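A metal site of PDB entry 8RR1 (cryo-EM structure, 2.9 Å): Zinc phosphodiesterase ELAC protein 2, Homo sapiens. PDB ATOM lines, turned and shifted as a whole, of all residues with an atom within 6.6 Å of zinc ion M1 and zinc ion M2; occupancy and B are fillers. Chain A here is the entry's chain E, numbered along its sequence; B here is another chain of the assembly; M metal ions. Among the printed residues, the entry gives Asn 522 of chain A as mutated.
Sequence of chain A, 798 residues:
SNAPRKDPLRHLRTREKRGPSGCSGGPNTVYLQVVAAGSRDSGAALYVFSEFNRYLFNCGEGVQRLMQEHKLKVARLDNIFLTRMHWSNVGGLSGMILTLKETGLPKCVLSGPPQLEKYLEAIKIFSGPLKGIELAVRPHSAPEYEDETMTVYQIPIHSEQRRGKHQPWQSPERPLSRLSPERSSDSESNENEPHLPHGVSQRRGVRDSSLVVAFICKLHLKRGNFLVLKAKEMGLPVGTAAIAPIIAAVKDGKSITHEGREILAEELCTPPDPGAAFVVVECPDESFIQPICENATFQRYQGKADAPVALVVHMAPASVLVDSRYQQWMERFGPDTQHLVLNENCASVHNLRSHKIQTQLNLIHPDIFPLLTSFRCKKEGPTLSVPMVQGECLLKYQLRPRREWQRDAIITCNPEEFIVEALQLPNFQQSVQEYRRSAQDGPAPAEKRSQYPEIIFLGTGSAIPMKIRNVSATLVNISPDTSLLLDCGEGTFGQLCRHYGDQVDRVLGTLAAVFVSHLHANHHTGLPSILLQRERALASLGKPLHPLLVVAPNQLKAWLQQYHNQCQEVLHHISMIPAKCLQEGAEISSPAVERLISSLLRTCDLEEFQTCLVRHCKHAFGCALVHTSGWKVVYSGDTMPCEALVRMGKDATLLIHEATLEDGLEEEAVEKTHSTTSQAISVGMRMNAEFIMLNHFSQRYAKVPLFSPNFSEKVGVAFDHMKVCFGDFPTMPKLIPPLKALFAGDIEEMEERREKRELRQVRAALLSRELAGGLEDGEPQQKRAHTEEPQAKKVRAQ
Within 4 Å of zinc ion M2: His 518, His 520, His 616 and Asp 638.
Along chain A the residues within 4 Å of zinc ion M2 span positions 518 to 638.
A ring nitrogen (NE2) of His 520 sits at hydrogen-bond distance from the side-chain sulfur of Cys 617, 3.5 Å away.
NE2 of His 523 lies close to OG of Ser 472, at 3.4 Å.
A ring nitrogen (NE2) of His 616 sits close to the side-chain sulfur (SG) of Cys 617, 3.8 Å away.
ND1 of His 616 is in hydrogen-bond range of O of Thr 673.
The side-chain carboxylate (OD2) of Asp 638 is bound to zinc ion M1 (2.1 Å).
NE2 of His 523 is bound to zinc ion M1, at 2.3 Å.
Zinc ion M1 is bound by a ring nitrogen (NE2) of His 696 (2.3 Å).
OD2 of Asp 638 binds zinc ion M2 (2.0 Å).
Zinc ion M2 is bound by ND1 of His 520.
A ring nitrogen (NE2) of His 518 is bound to zinc ion M2, 2.3 Å away.
A ring nitrogen (NE2) of His 616 binds zinc ion M2 (2.3 Å).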
ATOM      1  N   GLY A 461       8.043  14.170 -16.111  1.00  0.00           N
ATOM      2  CA  GLY A 461       8.345  14.204 -17.526  1.00  0.00           C
ATOM      3  C   GLY A 461       9.558  15.079 -17.782  1.00  0.00           C
ATOM      4  O   GLY A 461       9.893  15.973 -17.005  1.00  0.00           O
ATOM      5  N   SER A 462      10.228  14.801 -18.913  1.00  0.00           N
ATOM      6  CA  SER A 462      11.580  15.330 -19.080  1.00  0.00           C
ATOM      7  C   SER A 462      11.627  16.740 -19.636  1.00  0.00           C
ATOM      8  O   SER A 462      11.860  17.702 -18.890  1.00  0.00           O
ATOM      9  CB  SER A 462      12.385  14.409 -19.994  1.00  0.00           C
ATOM     10  OG  SER A 462      11.695  14.175 -21.210  1.00  0.00           O
ATOM     11  N   ALA A 463      11.422  16.897 -20.948  1.00  0.00           N
ATOM     12  CA  ALA A 463      11.613  18.210 -21.560  1.00  0.00           C
ATOM     13  C   ALA A 463      10.327  19.017 -21.711  1.00  0.00           C
ATOM     14  O   ALA A 463      10.105  19.986 -20.987  1.00  0.00           O
ATOM     15  CB  ALA A 463      12.278  18.045 -22.934  1.00  0.00           C
ATOM     16  N   SER A 472       9.531  18.089 -14.477  1.00  0.00           N
ATOM     17  CA  SER A 472       9.940  17.408 -13.260  1.00  0.00           C
ATOM     18  C   SER A 472       9.632  18.244 -12.024  1.00  0.00           C
ATOM     19  O   SER A 472       9.721  19.476 -12.035  1.00  0.00           O
ATOM     20  CB  SER A 472      11.432  17.083 -13.309  1.00  0.00           C
ATOM     21  OG  SER A 472      12.198  18.240 -13.637  1.00  0.00           O
ATOM     22  N   SER A 517      18.514  21.443  -9.192  1.00  0.00           N
ATOM     23  CA  SER A 517      19.636  20.620  -9.624  1.00  0.00           C
ATOM     24  C   SER A 517      19.878  20.896 -11.104  1.00  0.00           C
ATOM     25  O   SER A 517      19.124  20.420 -11.958  1.00  0.00           O
ATOM     26  CB  SER A 517      19.357  19.145  -9.366  1.00  0.00           C
ATOM     27  OG  SER A 517      18.162  18.745  -9.995  1.00  0.00           O
ATOM     28  N   HIS A 518      20.920  21.683 -11.389  1.00  0.00           N
ATOM     29  CA  HIS A 518      21.386  22.003 -12.742  1.00  0.00           C
ATOM     30  C   HIS A 518      20.395  22.909 -13.468  1.00  0.00           C
ATOM     31  O   HIS A 518      19.180  22.727 -13.365  1.00  0.00           O
ATOM     32  CB  HIS A 518      21.706  20.721 -13.532  1.00  0.00           C
ATOM     33  CG  HIS A 518      20.612  20.257 -14.444  1.00  0.00           C
ATOM     34  ND1 HIS A 518      19.426  19.724 -13.980  1.00  0.00           N
ATOM     35  CD2 HIS A 518      20.541  20.201 -15.801  1.00  0.00           C
ATOM     36  CE1 HIS A 518      18.662  19.393 -15.011  1.00  0.00           C
ATOM     37  NE2 HIS A 518      19.321  19.673 -16.120  1.00  0.00           N
ATOM     38  N   HIS A 520      19.131  23.633 -16.371  1.00  0.00           N
ATOM     39  CA  HIS A 520      18.340  23.433 -17.580  1.00  0.00           C
ATOM     40  C   HIS A 520      16.959  24.061 -17.410  1.00  0.00           C
ATOM     41  O   HIS A 520      16.443  24.177 -16.289  1.00  0.00           O
ATOM     42  CB  HIS A 520      18.188  21.951 -17.914  1.00  0.00           C
ATOM     43  CG  HIS A 520      19.330  21.404 -18.712  1.00  0.00           C
ATOM     44  ND1 HIS A 520      19.461  20.057 -18.996  1.00  0.00           N
ATOM     45  CD2 HIS A 520      20.377  22.016 -19.308  1.00  0.00           C
ATOM     46  CE1 HIS A 520      20.566  19.869 -19.709  1.00  0.00           C
ATOM     47  NE2 HIS A 520      21.128  21.037 -19.921  1.00  0.00           N
ATOM     48  N   ALA A 521      16.364  24.466 -18.519  1.00  0.00           N
ATOM     49  CA  ALA A 521      14.992  24.947 -18.493  1.00  0.00           C
ATOM     50  C   ALA A 521      14.065  23.828 -18.013  1.00  0.00           C
ATOM     51  O   ALA A 521      14.424  22.655 -17.977  1.00  0.00           O
ATOM     52  CB  ALA A 521      14.560  25.434 -19.865  1.00  0.00           C
ATOM     53  N   ASN A 522      12.855  24.238 -17.603  1.00  0.00           N
ATOM     54  CA  ASN A 522      11.801  23.341 -17.123  1.00  0.00           C
ATOM     55  C   ASN A 522      12.213  22.601 -15.863  1.00  0.00           C
ATOM     56  O   ASN A 522      11.462  21.759 -15.353  1.00  0.00           O
ATOM     57  CB  ASN A 522      11.380  22.356 -18.230  1.00  0.00           C
ATOM     58  CG  ASN A 522      12.073  21.013 -18.132  1.00  0.00           C
ATOM     59  OD1 ASN A 522      11.549  20.071 -17.529  1.00  0.00           O
ATOM     60  ND2 ASN A 522      13.258  20.916 -18.727  1.00  0.00           N
ATOM     61  N   HIS A 523      13.394  22.914 -15.318  1.00  0.00           N
ATOM     62  CA  HIS A 523      13.782  22.458 -13.998  1.00  0.00           C
ATOM     63  C   HIS A 523      13.763  23.559 -12.945  1.00  0.00           C
ATOM     64  O   HIS A 523      13.744  23.246 -11.753  1.00  0.00           O
ATOM     65  CB  HIS A 523      15.200  21.855 -14.031  1.00  0.00           C
ATOM     66  CG  HIS A 523      15.235  20.408 -14.425  1.00  0.00           C
ATOM     67  ND1 HIS A 523      15.661  19.413 -13.581  1.00  0.00           N
ATOM     68  CD2 HIS A 523      14.876  19.787 -15.582  1.00  0.00           C
ATOM     69  CE1 HIS A 523      15.583  18.244 -14.193  1.00  0.00           C
ATOM     70  NE2 HIS A 523      15.107  18.443 -15.412  1.00  0.00           N
ATOM     71  N   HIS A 616      26.131  15.140 -15.773  1.00  0.00           N
ATOM     72  CA  HIS A 616      25.121  15.482 -16.761  1.00  0.00           C
ATOM     73  C   HIS A 616      25.504  16.702 -17.589  1.00  0.00           C
ATOM     74  O   HIS A 616      25.501  16.647 -18.822  1.00  0.00           O
ATOM     75  CB  HIS A 616      23.766  15.723 -16.089  1.00  0.00           C
ATOM     76  CG  HIS A 616      22.738  16.343 -16.988  1.00  0.00           C
ATOM     77  ND1 HIS A 616      22.135  15.647 -18.022  1.00  0.00           N
ATOM     78  CD2 HIS A 616      22.207  17.583 -17.004  1.00  0.00           C
ATOM     79  CE1 HIS A 616      21.288  16.437 -18.640  1.00  0.00           C
ATOM     80  NE2 HIS A 616      21.310  17.617 -18.051  1.00  0.00           N
ATOM     81  N   CYS A 617      25.832  17.818 -16.935  1.00  0.00           N
ATOM     82  CA  CYS A 617      26.240  19.037 -17.605  1.00  0.00           C
ATOM     83  C   CYS A 617      27.222  19.761 -16.698  1.00  0.00           C
ATOM     84  O   CYS A 617      27.743  19.197 -15.735  1.00  0.00           O
ATOM     85  CB  CYS A 617      25.017  19.896 -17.955  1.00  0.00           C
ATOM     86  SG  CYS A 617      24.240  19.506 -19.540  1.00  0.00           S
ATOM     87  N   ASP A 638      18.954  14.917 -13.332  1.00  0.00           N
ATOM     88  CA  ASP A 638      19.563  14.612 -14.620  1.00  0.00           C
ATOM     89  C   ASP A 638      21.009  14.210 -14.416  1.00  0.00           C
ATOM     90  O   ASP A 638      21.793  14.962 -13.819  1.00  0.00           O
ATOM     91  CB  ASP A 638      19.463  15.825 -15.555  1.00  0.00           C
ATOM     92  CG  ASP A 638      18.031  16.174 -15.897  1.00  0.00           C
ATOM     93  OD1 ASP A 638      17.115  15.599 -15.277  1.00  0.00           O
ATOM     94  OD2 ASP A 638      17.819  17.022 -16.785  1.00  0.00           O
ATOM     95  N   THR A 639      21.378  13.015 -14.879  1.00  0.00           N
ATOM     96  CA  THR A 639      22.719  12.494 -14.657  1.00  0.00           C
ATOM     97  C   THR A 639      22.953  11.298 -15.569  1.00  0.00           C
ATOM     98  O   THR A 639      22.087  10.901 -16.347  1.00  0.00           O
ATOM     99  CB  THR A 639      22.955  12.092 -13.199  1.00  0.00           C
ATOM    100  OG1 THR A 639      24.284  11.589 -13.051  1.00  0.00           O
ATOM    101  CG2 THR A 639      21.982  11.005 -12.795  1.00  0.00           C
ATOM    102  N   GLU A 658      17.035   9.296 -12.430  1.00  0.00           N
ATOM    103  CA  GLU A 658      16.594   9.573 -13.786  1.00  0.00           C
ATOM    104  C   GLU A 658      16.515   8.293 -14.617  1.00  0.00           C
ATOM    105  O   GLU A 658      17.416   7.453 -14.559  1.00  0.00           O
ATOM    106  CB  GLU A 658      17.542  10.576 -14.449  1.00  0.00           C
ATOM    107  CG  GLU A 658      17.386  10.683 -15.945  1.00  0.00           C
ATOM    108  CD  GLU A 658      18.706  10.921 -16.645  1.00  0.00           C
ATOM    109  OE1 GLU A 658      19.332  11.963 -16.403  1.00  0.00           O
ATOM    110  OE2 GLU A 658      19.119  10.045 -17.434  1.00  0.00           O
ATOM    111  N   THR A 673      23.906  12.691 -22.518  1.00  0.00           N
ATOM    112  CA  THR A 673      24.227  12.725 -21.091  1.00  0.00           C
ATOM    113  C   THR A 673      22.981  12.404 -20.244  1.00  0.00           C
ATOM    114  O   THR A 673      22.489  13.219 -19.473  1.00  0.00           O
ATOM    115  CB  THR A 673      24.822  14.073 -20.691  1.00  0.00           C
ATOM    116  OG1 THR A 673      23.809  15.091 -20.695  1.00  0.00           O
ATOM    117  CG2 THR A 673      25.944  14.471 -21.645  1.00  0.00           C
ATOM    118  N   HIS A 674      22.492  11.186 -20.422  1.00  0.00           N
ATOM    119  CA  HIS A 674      21.343  10.688 -19.677  1.00  0.00           C
ATOM    120  C   HIS A 674      21.542   9.207 -19.377  1.00  0.00           C
ATOM    121  O   HIS A 674      22.397   8.544 -19.963  1.00  0.00           O
ATOM    122  CB  HIS A 674      20.040  10.916 -20.441  1.00  0.00           C
ATOM    123  CG  HIS A 674      19.431  12.273 -20.216  1.00  0.00           C
ATOM    124  ND1 HIS A 674      18.434  12.498 -19.298  1.00  0.00           N
ATOM    125  CD2 HIS A 674      19.690  13.461 -20.799  1.00  0.00           C
ATOM    126  CE1 HIS A 674      18.106  13.777 -19.317  1.00  0.00           C
ATOM    127  NE2 HIS A 674      18.848  14.387 -20.218  1.00  0.00           N
ATOM    128  N   HIS A 696      11.625  11.471 -14.582  1.00  0.00           N
ATOM    129  CA  HIS A 696      12.241  12.196 -15.694  1.00  0.00           C
ATOM    130  C   HIS A 696      12.151  11.402 -16.999  1.00  0.00           C
ATOM    131  O   HIS A 696      13.096  11.352 -17.784  1.00  0.00           O
ATOM    132  CB  HIS A 696      13.689  12.570 -15.379  1.00  0.00           C
ATOM    133  CG  HIS A 696      14.141  13.826 -16.047  1.00  0.00           C
ATOM    134  ND1 HIS A 696      14.633  13.853 -17.330  1.00  0.00           N
ATOM    135  CD2 HIS A 696      14.187  15.103 -15.595  1.00  0.00           C
ATOM    136  CE1 HIS A 696      14.960  15.092 -17.650  1.00  0.00           C
ATOM    137  NE2 HIS A 696      14.692  15.873 -16.619  1.00  0.00           N
ATOM    138  P     A B  66      15.274  16.890 -29.183  1.00  0.00           P
ATOM    139  OP1   A B  66      16.645  16.292 -29.386  1.00  0.00           O
ATOM    140  OP2   A B  66      14.470  16.234 -28.074  1.00  0.00           O
ATOM    141  O5'   A B  66      15.480  18.450 -28.791  1.00  0.00           O
ATOM    142  C5'   A B  66      15.094  18.945 -27.469  1.00  0.00           C
ATOM    143  C4'   A B  66      16.027  18.402 -26.421  1.00  0.00           C
ATOM    144  O4'   A B  66      17.180  17.786 -27.058  1.00  0.00           O
ATOM    145  C3'   A B  66      16.672  19.406 -25.456  1.00  0.00           C
ATOM    146  O3'   A B  66      15.832  19.878 -24.410  1.00  0.00           O
ATOM    147  C2'   A B  66      17.832  18.541 -24.953  1.00  0.00           C
ATOM    148  O2'   A B  66      17.427  17.511 -24.083  1.00  0.00           O
ATOM    149  C1'   A B  66      18.332  18.004 -26.290  1.00  0.00           C
ATOM    150  N9    A B  66      19.191  18.967 -26.969  1.00  0.00           N
ATOM    151  C8    A B  66      20.303  19.566 -26.420  1.00  0.00           C
ATOM    152  N7    A B  66      20.911  20.383 -27.235  1.00  0.00           N
ATOM    153  C5    A B  66      20.158  20.324 -28.403  1.00  0.00           C
ATOM    154  C6    A B  66      20.298  20.971 -29.633  1.00  0.00           C
ATOM    155  N6    A B  66      21.278  21.835 -29.914  1.00  0.00           N
ATOM    156  N1    A B  66      19.386  20.684 -30.596  1.00  0.00           N
ATOM    157  C2    A B  66      18.408  19.825 -30.307  1.00  0.00           C
ATOM    158  N3    A B  66      18.181  19.159 -29.184  1.00  0.00           N
ATOM    159  C4    A B  66      19.112  19.440 -28.259  1.00  0.00           C
ATOM    160  P     G B  67      16.445  20.690 -23.162  1.00  0.00           P
ATOM    161  OP1   G B  67      16.813  19.731 -22.048  1.00  0.00           O
ATOM    162  OP2   G B  67      15.574  21.838 -22.699  1.00  0.00           O
ATOM    163  O5'   G B  67      17.824  21.327 -23.724  1.00  0.00           O
ATOM    164  C5'   G B  67      18.156  22.710 -23.427  1.00  0.00           C
ATOM    165  C4'   G B  67      19.372  23.122 -24.221  1.00  0.00           C
ATOM    166  O4'   G B  67      19.144  22.774 -25.612  1.00  0.00           O
ATOM    167  C3'   G B  67      19.691  24.619 -24.227  1.00  0.00           C
ATOM    168  O3'   G B  67      21.056  24.948 -24.489  1.00  0.00           O
ATOM    169  C2'   G B  67      18.844  25.110 -25.415  1.00  0.00           C
ATOM    170  O2'   G B  67      19.347  26.287 -25.998  1.00  0.00           O
ATOM    171  C1'   G B  67      18.968  23.948 -26.381  1.00  0.00           C
ATOM    172  N9    G B  67      17.789  23.781 -27.219  1.00  0.00           N
ATOM    173  C8    G B  67      16.669  23.041 -26.941  1.00  0.00           C
ATOM    174  N7    G B  67      15.771  23.089 -27.886  1.00  0.00           N
ATOM    175  C5    G B  67      16.327  23.919 -28.851  1.00  0.00           C
ATOM    176  C6    G B  67      15.812  24.345 -30.089  1.00  0.00           C
ATOM    177  O6    G B  67      14.718  24.062 -30.608  1.00  0.00           O
ATOM    178  N1    G B  67      16.695  25.179 -30.754  1.00  0.00           N
ATOM    179  C2    G B  67      17.925  25.561 -30.281  1.00  0.00           C
ATOM    180  N2    G B  67      18.642  26.380 -31.080  1.00  0.00           N
ATOM    181  N3    G B  67      18.423  25.168 -29.113  1.00  0.00           N
ATOM    182  C4    G B  67      17.565  24.352 -28.453  1.00  0.00           C
HETATM  183 ZN    ZN M   1      15.952  17.639 -17.392  1.00  0.00          ZN
HETATM  184 ZN    ZN M   2      19.084  18.137 -17.811  1.00  0.00          ZN
